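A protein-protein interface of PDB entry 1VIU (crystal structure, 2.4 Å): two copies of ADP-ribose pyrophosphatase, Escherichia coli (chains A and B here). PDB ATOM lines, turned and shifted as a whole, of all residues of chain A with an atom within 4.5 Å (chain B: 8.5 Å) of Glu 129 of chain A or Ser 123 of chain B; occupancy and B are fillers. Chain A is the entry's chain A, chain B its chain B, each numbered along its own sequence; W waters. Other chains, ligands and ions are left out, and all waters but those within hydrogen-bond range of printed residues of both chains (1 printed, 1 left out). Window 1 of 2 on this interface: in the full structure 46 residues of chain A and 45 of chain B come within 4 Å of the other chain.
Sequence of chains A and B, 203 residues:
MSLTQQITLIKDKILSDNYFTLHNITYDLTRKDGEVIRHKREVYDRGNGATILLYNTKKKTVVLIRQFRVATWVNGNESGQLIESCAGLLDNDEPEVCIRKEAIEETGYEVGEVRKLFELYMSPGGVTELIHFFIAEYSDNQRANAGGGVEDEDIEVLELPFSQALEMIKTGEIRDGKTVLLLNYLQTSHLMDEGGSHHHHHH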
ATOM      1  N   ARG A  46     -14.982 -21.806  22.071  1.00  0.00           N
ATOM      2  CA  ARG A  46     -15.207 -23.140  22.611  1.00  0.00           C
ATOM      3  C   ARG A  46     -14.067 -24.068  22.191  1.00  0.00           C
ATOM      4  O   ARG A  46     -14.213 -25.279  22.180  1.00  0.00           O
ATOM      5  CB  ARG A  46     -16.556 -23.700  22.135  1.00  0.00           C
ATOM      6  CG  ARG A  46     -16.748 -23.651  20.642  1.00  0.00           C
ATOM      7  CD  ARG A  46     -18.154 -24.061  20.232  1.00  0.00           C
ATOM      8  NE  ARG A  46     -18.421 -25.493  20.387  1.00  0.00           N
ATOM      9  CZ  ARG A  46     -18.998 -26.040  21.452  1.00  0.00           C
ATOM     10  NH1 ARG A  46     -19.373 -25.278  22.472  1.00  0.00           N
ATOM     11  NH2 ARG A  46     -19.233 -27.344  21.480  1.00  0.00           N
ATOM     12  N   GLY A  47     -12.925 -23.487  21.852  1.00  0.00           N
ATOM     13  CA  GLY A  47     -11.794 -24.296  21.441  1.00  0.00           C
ATOM     14  C   GLY A  47     -11.960 -24.852  20.036  1.00  0.00           C
ATOM     15  O   GLY A  47     -13.039 -24.784  19.444  1.00  0.00           O
ATOM     16  N   ASN A  48     -10.886 -25.408  19.495  1.00  0.00           N
ATOM     17  CA  ASN A  48     -10.931 -25.967  18.161  1.00  0.00           C
ATOM     18  C   ASN A  48     -11.242 -27.460  18.194  1.00  0.00           C
ATOM     19  O   ASN A  48     -11.218 -28.094  19.253  1.00  0.00           O
ATOM     20  CB  ASN A  48      -9.607 -25.695  17.449  1.00  0.00           C
ATOM     21  CG  ASN A  48      -9.288 -24.215  17.377  1.00  0.00           C
ATOM     22  OD1 ASN A  48     -10.146 -23.395  17.033  1.00  0.00           O
ATOM     23  ND2 ASN A  48      -8.053 -23.862  17.690  1.00  0.00           N
ATOM     24  N   LEU A 120     -10.317 -25.063   8.784  1.00  0.00           N
ATOM     25  CA  LEU A 120     -11.156 -23.915   8.477  1.00  0.00           C
ATOM     26  C   LEU A 120     -11.893 -23.345   9.679  1.00  0.00           C
ATOM     27  O   LEU A 120     -12.254 -24.077  10.610  1.00  0.00           O
ATOM     28  CB  LEU A 120     -12.188 -24.296   7.399  1.00  0.00           C
ATOM     29  CG  LEU A 120     -11.677 -25.078   6.178  1.00  0.00           C
ATOM     30  CD1 LEU A 120     -12.849 -25.480   5.293  1.00  0.00           C
ATOM     31  CD2 LEU A 120     -10.661 -24.246   5.397  1.00  0.00           C
ATOM     32  N   TYR A 121     -12.090 -22.029   9.646  1.00  0.00           N
ATOM     33  CA  TYR A 121     -12.848 -21.329  10.669  1.00  0.00           C
ATOM     34  C   TYR A 121     -14.302 -21.559  10.236  1.00  0.00           C
ATOM     35  O   TYR A 121     -14.638 -21.350   9.070  1.00  0.00           O
ATOM     36  CB  TYR A 121     -12.496 -19.837  10.658  1.00  0.00           C
ATOM     37  CG  TYR A 121     -11.108 -19.558  11.182  1.00  0.00           C
ATOM     38  CD1 TYR A 121     -10.077 -19.180  10.327  1.00  0.00           C
ATOM     39  CD2 TYR A 121     -10.816 -19.721  12.533  1.00  0.00           C
ATOM     40  CE1 TYR A 121      -8.785 -18.973  10.810  1.00  0.00           C
ATOM     41  CE2 TYR A 121      -9.541 -19.519  13.025  1.00  0.00           C
ATOM     42  CZ  TYR A 121      -8.530 -19.142  12.166  1.00  0.00           C
ATOM     43  OH  TYR A 121      -7.275 -18.920  12.677  1.00  0.00           O
ATOM     44  N   MET A 122     -15.160 -22.000  11.152  1.00  0.00           N
ATOM     45  CA  MET A 122     -16.543 -22.294  10.785  1.00  0.00           C
ATOM     46  C   MET A 122     -17.559 -21.159  10.936  1.00  0.00           C
ATOM     47  O   MET A 122     -18.591 -21.145  10.261  1.00  0.00           O
ATOM     48  CB  MET A 122     -17.012 -23.537  11.547  1.00  0.00           C
ATOM     49  CG  MET A 122     -16.189 -24.785  11.224  1.00  0.00           C
ATOM     50  SD  MET A 122     -16.168 -25.231   9.294  1.00  0.00           S
ATOM     51  CE  MET A 122     -17.863 -26.160   9.192  1.00  0.00           C
ATOM     52  N   VAL A 127     -17.310 -16.499  16.487  1.00  0.00           N
ATOM     53  CA  VAL A 127     -16.819 -17.740  17.058  1.00  0.00           C
ATOM     54  C   VAL A 127     -15.390 -18.000  16.602  1.00  0.00           C
ATOM     55  O   VAL A 127     -15.088 -17.881  15.417  1.00  0.00           O
ATOM     56  CB  VAL A 127     -17.706 -18.928  16.620  1.00  0.00           C
ATOM     57  CG1 VAL A 127     -17.323 -20.166  17.398  1.00  0.00           C
ATOM     58  CG2 VAL A 127     -19.179 -18.578  16.830  1.00  0.00           C
ATOM     59  N   THR A 128     -14.514 -18.364  17.535  1.00  0.00           N
ATOM     60  CA  THR A 128     -13.121 -18.625  17.189  1.00  0.00           C
ATOM     61  C   THR A 128     -12.934 -19.969  16.483  1.00  0.00           C
ATOM     62  O   THR A 128     -11.980 -20.147  15.729  1.00  0.00           O
ATOM     63  CB  THR A 128     -12.202 -18.644  18.447  1.00  0.00           C
ATOM     64  OG1 THR A 128     -12.626 -19.683  19.340  1.00  0.00           O
ATOM     65  CG2 THR A 128     -12.242 -17.312  19.173  1.00  0.00           C
ATOM     66  N   GLU A 129     -13.866 -20.892  16.709  1.00  0.00           N
ATOM     67  CA  GLU A 129     -13.773 -22.243  16.181  1.00  0.00           C
ATOM     68  C   GLU A 129     -13.113 -22.490  14.831  1.00  0.00           C
ATOM     69  O   GLU A 129     -13.534 -21.973  13.792  1.00  0.00           O
ATOM     70  CB  GLU A 129     -15.145 -22.931  16.195  1.00  0.00           C
ATOM     71  CG  GLU A 129     -15.048 -24.463  16.008  1.00  0.00           C
ATOM     72  CD  GLU A 129     -16.406 -25.160  15.875  1.00  0.00           C
ATOM     73  OE1 GLU A 129     -17.150 -24.857  14.925  1.00  0.00           O
ATOM     74  OE2 GLU A 129     -16.731 -26.022  16.720  1.00  0.00           O
ATOM     75  N   LEU A 130     -12.072 -23.319  14.888  1.00  0.00           N
ATOM     76  CA  LEU A 130     -11.297 -23.759  13.731  1.00  0.00           C
ATOM     77  C   LEU A 130     -11.402 -25.289  13.761  1.00  0.00           C
ATOM     78  O   LEU A 130     -11.161 -25.913  14.801  1.00  0.00           O
ATOM     79  CB  LEU A 130      -9.835 -23.329  13.884  1.00  0.00           C
ATOM     80  CG  LEU A 130      -8.768 -23.704  12.843  1.00  0.00           C
ATOM     81  CD1 LEU A 130      -9.034 -23.015  11.512  1.00  0.00           C
ATOM     82  CD2 LEU A 130      -7.403 -23.269  13.371  1.00  0.00           C
ATOM     83  N   ILE A 131     -11.802 -25.888  12.646  1.00  0.00           N
ATOM     84  CA  ILE A 131     -11.928 -27.341  12.567  1.00  0.00           C
ATOM     85  C   ILE A 131     -10.900 -27.951  11.611  1.00  0.00           C
ATOM     86  O   ILE A 131     -10.691 -27.447  10.496  1.00  0.00           O
ATOM     87  CB  ILE A 131     -13.330 -27.780  12.079  1.00  0.00           C
ATOM     88  CG1 ILE A 131     -14.398 -27.371  13.099  1.00  0.00           C
ATOM     89  CG2 ILE A 131     -13.358 -29.305  11.873  1.00  0.00           C
ATOM     90  CD1 ILE A 131     -14.149 -27.920  14.487  1.00  0.00           C
ATOM     91  N   GLU B  42     -23.960 -25.239  26.772  1.00  0.00           N
ATOM     92  CA  GLU B  42     -23.942 -23.844  26.423  1.00  0.00           C
ATOM     93  C   GLU B  42     -24.381 -23.714  24.986  1.00  0.00           C
ATOM     94  O   GLU B  42     -23.948 -24.471  24.129  1.00  0.00           O
ATOM     95  CB  GLU B  42     -22.534 -23.264  26.581  1.00  0.00           C
ATOM     96  CG  GLU B  42     -22.229 -22.716  27.964  1.00  0.00           C
ATOM     97  CD  GLU B  42     -20.797 -22.228  28.104  1.00  0.00           C
ATOM     98  OE1 GLU B  42     -20.212 -21.747  27.105  1.00  0.00           O
ATOM     99  OE2 GLU B  42     -20.256 -22.315  29.225  1.00  0.00           O
ATOM    100  N   VAL B  43     -25.261 -22.756  24.738  1.00  0.00           N
ATOM    101  CA  VAL B  43     -25.735 -22.491  23.401  1.00  0.00           C
ATOM    102  C   VAL B  43     -25.577 -20.995  23.142  1.00  0.00           C
ATOM    103  O   VAL B  43     -26.148 -20.150  23.846  1.00  0.00           O
ATOM    104  CB  VAL B  43     -27.218 -22.876  23.227  1.00  0.00           C
ATOM    105  CG1 VAL B  43     -27.678 -22.512  21.821  1.00  0.00           C
ATOM    106  CG2 VAL B  43     -27.413 -24.373  23.500  1.00  0.00           C
ATOM    107  N   TYR B  44     -24.772 -20.671  22.144  1.00  0.00           N
ATOM    108  CA  TYR B  44     -24.557 -19.287  21.782  1.00  0.00           C
ATOM    109  C   TYR B  44     -25.453 -19.064  20.583  1.00  0.00           C
ATOM    110  O   TYR B  44     -25.360 -19.785  19.589  1.00  0.00           O
ATOM    111  CB  TYR B  44     -23.101 -19.055  21.409  1.00  0.00           C
ATOM    112  CG  TYR B  44     -22.766 -17.620  21.158  1.00  0.00           C
ATOM    113  CD1 TYR B  44     -23.165 -16.623  22.053  1.00  0.00           C
ATOM    114  CD2 TYR B  44     -22.007 -17.250  20.054  1.00  0.00           C
ATOM    115  CE1 TYR B  44     -22.811 -15.302  21.854  1.00  0.00           C
ATOM    116  CE2 TYR B  44     -21.641 -15.924  19.845  1.00  0.00           C
ATOM    117  CZ  TYR B  44     -22.048 -14.955  20.748  1.00  0.00           C
ATOM    118  OH  TYR B  44     -21.678 -13.646  20.550  1.00  0.00           O
ATOM    119  N   ALA B  71     -12.251 -12.799  16.043  1.00  0.00           N
ATOM    120  CA  ALA B  71     -12.398 -14.190  16.432  1.00  0.00           C
ATOM    121  C   ALA B  71     -11.248 -15.076  15.917  1.00  0.00           C
ATOM    122  O   ALA B  71     -10.802 -15.980  16.629  1.00  0.00           O
ATOM    123  CB  ALA B  71     -13.754 -14.726  15.969  1.00  0.00           C
ATOM    124  N   THR B  72     -10.758 -14.814  14.703  1.00  0.00           N
ATOM    125  CA  THR B  72      -9.651 -15.598  14.155  1.00  0.00           C
ATOM    126  C   THR B  72      -8.297 -15.062  14.604  1.00  0.00           C
ATOM    127  O   THR B  72      -7.362 -15.834  14.829  1.00  0.00           O
ATOM    128  CB  THR B  72      -9.658 -15.642  12.602  1.00  0.00           C
ATOM    129  OG1 THR B  72      -9.268 -14.368  12.068  1.00  0.00           O
ATOM    130  CG2 THR B  72     -11.040 -16.010  12.088  1.00  0.00           C
ATOM    131  N   VAL B  74      -7.421 -13.890  17.441  1.00  0.00           N
ATOM    132  CA  VAL B  74      -7.059 -14.386  18.757  1.00  0.00           C
ATOM    133  C   VAL B  74      -6.962 -15.903  18.738  1.00  0.00           C
ATOM    134  O   VAL B  74      -6.808 -16.538  19.786  1.00  0.00           O
ATOM    135  CB  VAL B  74      -8.094 -13.963  19.819  1.00  0.00           C
ATOM    136  CG1 VAL B  74      -8.337 -12.458  19.722  1.00  0.00           C
ATOM    137  CG2 VAL B  74      -9.390 -14.748  19.635  1.00  0.00           C
ATOM    138  N   ASN B  75      -7.046 -16.482  17.544  1.00  0.00           N
ATOM    139  CA  ASN B  75      -6.971 -17.926  17.407  1.00  0.00           C
ATOM    140  C   ASN B  75      -6.197 -18.378  16.174  1.00  0.00           C
ATOM    141  O   ASN B  75      -6.754 -19.022  15.280  1.00  0.00           O
ATOM    142  CB  ASN B  75      -8.384 -18.526  17.394  1.00  0.00           C
ATOM    143  CG  ASN B  75      -8.380 -20.046  17.487  1.00  0.00           C
ATOM    144  OD1 ASN B  75      -7.608 -20.629  18.249  1.00  0.00           O
ATOM    145  ND2 ASN B  75      -9.260 -20.694  16.723  1.00  0.00           N
ATOM    146  N   LEU B 120     -27.463 -24.453   6.224  1.00  0.00           N
ATOM    147  CA  LEU B 120     -26.619 -25.302   7.059  1.00  0.00           C
ATOM    148  C   LEU B 120     -26.171 -24.732   8.402  1.00  0.00           C
ATOM    149  O   LEU B 120     -25.836 -23.546   8.522  1.00  0.00           O
ATOM    150  CB  LEU B 120     -25.352 -25.708   6.280  1.00  0.00           C
ATOM    151  CG  LEU B 120     -25.481 -26.173   4.821  1.00  0.00           C
ATOM    152  CD1 LEU B 120     -24.080 -26.413   4.268  1.00  0.00           C
ATOM    153  CD2 LEU B 120     -26.336 -27.446   4.712  1.00  0.00           C
ATOM    154  N   TYR B 121     -26.165 -25.601   9.410  1.00  0.00           N
ATOM    155  CA  TYR B 121     -25.673 -25.230  10.727  1.00  0.00           C
ATOM    156  C   TYR B 121     -24.145 -25.305  10.550  1.00  0.00           C
ATOM    157  O   TYR B 121     -23.623 -26.315  10.090  1.00  0.00           O
ATOM    158  CB  TYR B 121     -26.161 -26.233  11.783  1.00  0.00           C
ATOM    159  CG  TYR B 121     -27.662 -26.188  11.980  1.00  0.00           C
ATOM    160  CD1 TYR B 121     -28.492 -27.134  11.391  1.00  0.00           C
ATOM    161  CD2 TYR B 121     -28.256 -25.163  12.719  1.00  0.00           C
ATOM    162  CE1 TYR B 121     -29.875 -27.061  11.527  1.00  0.00           C
ATOM    163  CE2 TYR B 121     -29.635 -25.080  12.861  1.00  0.00           C
ATOM    164  CZ  TYR B 121     -30.442 -26.031  12.266  1.00  0.00           C
ATOM    165  OH  TYR B 121     -31.814 -25.951  12.406  1.00  0.00           O
ATOM    166  N   MET B 122     -23.435 -24.236  10.884  1.00  0.00           N
ATOM    167  CA  MET B 122     -21.984 -24.209  10.712  1.00  0.00           C
ATOM    168  C   MET B 122     -21.197 -24.700  11.921  1.00  0.00           C
ATOM    169  O   MET B 122     -20.061 -25.155  11.782  1.00  0.00           O
ATOM    170  CB  MET B 122     -21.535 -22.787  10.344  1.00  0.00           C
ATOM    171  CG  MET B 122     -22.086 -22.290   9.010  1.00  0.00           C
ATOM    172  SD  MET B 122     -21.604 -23.438   7.522  1.00  0.00           S
ATOM    173  CE  MET B 122     -19.762 -22.868   7.314  1.00  0.00           C
ATOM    174  N   SER B 123     -21.798 -24.613  13.101  1.00  0.00           N
ATOM    175  CA  SER B 123     -21.128 -25.044  14.325  1.00  0.00           C
ATOM    176  C   SER B 123     -22.210 -25.438  15.336  1.00  0.00           C
ATOM    177  O   SER B 123     -22.368 -24.804  16.364  1.00  0.00           O
ATOM    178  CB  SER B 123     -20.275 -23.886  14.857  1.00  0.00           C
ATOM    179  OG  SER B 123     -19.452 -24.296  15.934  1.00  0.00           O
ATOM    180  N   PRO B 124     -22.955 -26.517  15.046  1.00  0.00           N
ATOM    181  CA  PRO B 124     -24.052 -27.073  15.842  1.00  0.00           C
ATOM    182  C   PRO B 124     -23.703 -27.566  17.239  1.00  0.00           C
ATOM    183  O   PRO B 124     -24.598 -27.906  18.023  1.00  0.00           O
ATOM    184  CB  PRO B 124     -24.559 -28.204  14.958  1.00  0.00           C
ATOM    185  CG  PRO B 124     -23.287 -28.743  14.419  1.00  0.00           C
ATOM    186  CD  PRO B 124     -22.580 -27.467  13.979  1.00  0.00           C
ATOM    187  N   GLY B 125     -22.409 -27.622  17.535  1.00  0.00           N
ATOM    188  CA  GLY B 125     -21.964 -28.087  18.833  1.00  0.00           C
ATOM    189  C   GLY B 125     -22.301 -27.121  19.953  1.00  0.00           C
ATOM    190  O   GLY B 125     -22.574 -27.544  21.074  1.00  0.00           O
ATOM    191  N   GLY B 126     -22.281 -25.823  19.662  1.00  0.00           N
ATOM    192  CA  GLY B 126     -22.596 -24.847  20.690  1.00  0.00           C
ATOM    193  C   GLY B 126     -23.149 -23.543  20.145  1.00  0.00           C
ATOM    194  O   GLY B 126     -23.308 -22.588  20.885  1.00  0.00           O
ATOM    195  N   VAL B 127     -23.440 -23.511  18.850  1.00  0.00           N
ATOM    196  CA  VAL B 127     -23.962 -22.318  18.203  1.00  0.00           C
ATOM    197  C   VAL B 127     -25.218 -22.656  17.390  1.00  0.00           C
ATOM    198  O   VAL B 127     -25.261 -23.659  16.672  1.00  0.00           O
ATOM    199  CB  VAL B 127     -22.905 -21.697  17.261  1.00  0.00           C
ATOM    200  CG1 VAL B 127     -23.340 -20.298  16.830  1.00  0.00           C
ATOM    201  CG2 VAL B 127     -21.562 -21.651  17.956  1.00  0.00           C
ATOM    202  N   THR B 128     -26.237 -21.818  17.515  1.00  0.00           N
ATOM    203  CA  THR B 128     -27.501 -22.020  16.815  1.00  0.00           C
ATOM    204  C   THR B 128     -27.372 -21.655  15.341  1.00  0.00           C
ATOM    205  O   THR B 128     -28.083 -22.185  14.501  1.00  0.00           O
ATOM    206  CB  THR B 128     -28.614 -21.118  17.406  1.00  0.00           C
ATOM    207  OG1 THR B 128     -28.159 -19.756  17.402  1.00  0.00           O
ATOM    208  CG2 THR B 128     -28.956 -21.516  18.829  1.00  0.00           C
ATOM    209  N   GLU B 129     -26.448 -20.749  15.038  1.00  0.00           N
ATOM    210  CA  GLU B 129     -26.248 -20.237  13.686  1.00  0.00           C
ATOM    211  C   GLU B 129     -26.530 -21.145  12.486  1.00  0.00           C
ATOM    212  O   GLU B 129     -25.902 -22.194  12.303  1.00  0.00           O
ATOM    213  CB  GLU B 129     -24.833 -19.660  13.541  1.00  0.00           C
ATOM    214  CG  GLU B 129     -24.620 -18.888  12.236  1.00  0.00           C
ATOM    215  CD  GLU B 129     -23.164 -18.523  11.983  1.00  0.00           C
ATOM    216  OE1 GLU B 129     -22.339 -19.439  11.776  1.00  0.00           O
ATOM    217  OE2 GLU B 129     -22.840 -17.316  11.986  1.00  0.00           O
ATOM    218  N   LEU B 130     -27.479 -20.697  11.666  1.00  0.00           N
ATOM    219  CA  LEU B 130     -27.858 -21.366  10.427  1.00  0.00           C
ATOM    220  C   LEU B 130     -27.498 -20.392   9.291  1.00  0.00           C
ATOM    221  O   LEU B 130     -27.851 -19.211   9.342  1.00  0.00           O
ATOM    222  CB  LEU B 130     -29.365 -21.629  10.406  1.00  0.00           C
ATOM    223  CG  LEU B 130     -29.951 -22.238   9.127  1.00  0.00           C
ATOM    224  CD1 LEU B 130     -29.473 -23.691   8.961  1.00  0.00           C
ATOM    225  CD2 LEU B 130     -31.477 -22.179   9.199  1.00  0.00           C
ATOM    226  N   ILE B 131     -26.786 -20.868   8.278  1.00  0.00           N
ATOM    227  CA  ILE B 131     -26.425 -20.010   7.150  1.00  0.00           C
ATOM    228  C   ILE B 131     -27.103 -20.432   5.848  1.00  0.00           C
ATOM    229  O   ILE B 131     -27.046 -21.601   5.466  1.00  0.00           O
ATOM    230  CB  ILE B 131     -24.900 -19.992   6.900  1.00  0.00           C
ATOM    231  CG1 ILE B 131     -24.176 -19.408   8.118  1.00  0.00           C
ATOM    232  CG2 ILE B 131     -24.585 -19.181   5.641  1.00  0.00           C
ATOM    233  CD1 ILE B 131     -24.746 -18.092   8.596  1.00  0.00           C
ATOM    234  N   ARG B 175      -9.325 -19.955   4.038  1.00  0.00           N
ATOM    235  CA  ARG B 175      -9.605 -20.964   5.044  1.00  0.00           C
ATOM    236  C   ARG B 175     -10.894 -20.704   5.816  1.00  0.00           C
ATOM    237  O   ARG B 175     -10.971 -20.919   7.021  1.00  0.00           O
ATOM    238  CB  ARG B 175      -8.419 -21.078   5.998  1.00  0.00           C
ATOM    239  CG  ARG B 175      -7.921 -19.750   6.499  1.00  0.00           C
ATOM    240  CD  ARG B 175      -6.605 -19.915   7.226  1.00  0.00           C
ATOM    241  NE  ARG B 175      -6.072 -18.626   7.647  1.00  0.00           N
ATOM    242  CZ  ARG B 175      -4.801 -18.416   7.967  1.00  0.00           C
ATOM    243  NH1 ARG B 175      -4.403 -17.208   8.341  1.00  0.00           N
ATOM    244  NH2 ARG B 175      -3.927 -19.412   7.903  1.00  0.00           N
ATOM    245  N   ASP B 176     -11.908 -20.235   5.107  1.00  0.00           N
ATOM    246  CA  ASP B 176     -13.196 -19.976   5.717  1.00  0.00           C
ATOM    247  C   ASP B 176     -14.211 -21.020   5.261  1.00  0.00           C
ATOM    248  O   ASP B 176     -14.420 -21.205   4.066  1.00  0.00           O
ATOM    249  CB  ASP B 176     -13.694 -18.583   5.346  1.00  0.00           C
ATOM    250  CG  ASP B 176     -15.105 -18.349   5.809  1.00  0.00           C
ATOM    251  OD1 ASP B 176     -15.990 -18.191   4.947  1.00  0.00           O
ATOM    252  OD2 ASP B 176     -15.333 -18.350   7.039  1.00  0.00           O
ATOM    253  N   GLY B 177     -14.840 -21.687   6.222  1.00  0.00           N
ATOM    254  CA  GLY B 177     -15.817 -22.719   5.918  1.00  0.00           C
ATOM    255  C   GLY B 177     -16.872 -22.442   4.857  1.00  0.00           C
ATOM    256  O   GLY B 177     -17.010 -23.210   3.907  1.00  0.00           O
HETATM  257  O   HOH W   1     -18.080 -26.500  13.148  1.00  0.00           O
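The side-chain carboxylate (OE1) of Glu 129 of chain A sits at hydrogen-bond distance from the side-chain hydroxyl (OG) of Ser 123 of chain B (2.6 Å). The backbone NH (N) of Gly 177 of chain B sits at hydrogen-bond distance from the backbone carbonyl oxygen (O) of Tyr 121 of chain A, at 2.9 Å. The backbone NH (N) of Tyr 121 of chain A is in hydrogen-bond range of the backbone carbonyl oxygen (O) of Arg 175 of chain B (3.1 Å). The backbone carbonyl oxygen (O) of Thr 128 of chain A sits at hydrogen-bond distance from the side-chain amide nitrogen (ND2) of Asn 75 of chain B, at 2.9 Å. OD1 of Asn 48 of chain A sits at hydrogen-bond distance from ND2 of Asn 75 of chain B. The backbone carbonyl oxygen (O) of Asn 75 of chain B is in hydrogen-bond range of the side-chain hydroxyl (OH) of Tyr 121 of chain A (2.7 Å). The guanidinium group (NH2) of Arg 46 of chain A is in hydrogen-bond range of the backbone carbonyl oxygen (O) of Gly 125 of chain B (3.4 Å).
OD1 of Asn 48 of chain A is in hydrogen-bond range of N of Leu 130 of chain A, at 2.9 Å. N of Ile 131 of chain A lies within hydrogen-bond range of O of Leu 120 of chain A (2.8 Å). N of Tyr 44 of chain B sits at hydrogen-bond distance from O of Gly 126 of chain B. N of Met 122 of chain A is in hydrogen-bond range of O of Glu 129 of chain A, 3.1 Å away.
NH1 of Arg 46 of chain A touches CA of Gly 126 of chain B, at 3.7 Å. O of Arg 175 of chain B touches CA of Leu 120 of chain A, 3.3 Å away. Gly 177 of chain B touches Leu 120 of chain A. Tyr 121 of chain A touches Thr 72 of chain B (CG to CG2, 3.7 Å). OD2 of Asp 176 of chain B touches O of Tyr 121 of chain A (3.7 Å). Met 122 of chain B touches Met 122 of chain A (CB to O, 3.4 Å). O of Val 127 of chain A touches CB of Ala 71 of chain B (3.5 Å). O of Ala 71 of chain B touches CG2 of Thr 128 of chain A, 3.2 Å away. Val 74 of chain B touches Thr 128 of chain A. Leu 130 of chain A touches Asn 75 of chain B.
Glu 129 of chain A touches just one residue of chain B: Ser 123 (2.6 Å). Printed residues of chain B within 4 Å of Met 122 of chain A: Met 122 (3.4 Å). Printed residues of chain A within 4 Å of Ala 71 of chain B: Val 127 and Thr 128. Of the printed residues of chain A, Gly 125 of chain B touches Arg 46 (3.4 Å). Of the printed residues of chain A, Asp 176 of chain B touches Tyr 121 (3.7 Å). Of the printed residues of chain A, Gly 126 of chain B touches Arg 46 (3.7 Å). Ile 131 of chain B touches none of the printed residues of chain A. Gly 47 of chain A touches none of the printed residues of chain B. The nearest printed residue of chain A that does not touch Thr 72 of chain B is Thr 128 of chain A (5.1 Å).
Of the 11 printed residues of chain A, 9 touch a printed residue of chain B. Printed residues of chain A that touch a printed residue of chain B: Arg 46, Asn 48, Leu 120, Tyr 121, Met 122, Val 127, Thr 128, Glu 129 and Leu 130. Hydrophobic or aromatic side chains of chain A that line the printed part of chain B: Leu 120, Tyr 121, Met 122 and Leu 130. Of the 22 printed residues of chain B, 11 touch a printed residue of chain A. Among the printed residues, 17 pairs touch across the chains.
Met 122 of chain A touches its own counterpart, Met 122 of chain B. Positions printed for both chains: 120, 121, 122, 127, 128, 129, 130 and 131. Of the 17 pairs that touch across the chains among the printed residues, 1 has its exchanged pair printed and touching as well.
Water W1 lies within hydrogen-bond range of OE1 of Glu 129 of chain A and O of Met 122 of chain B.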
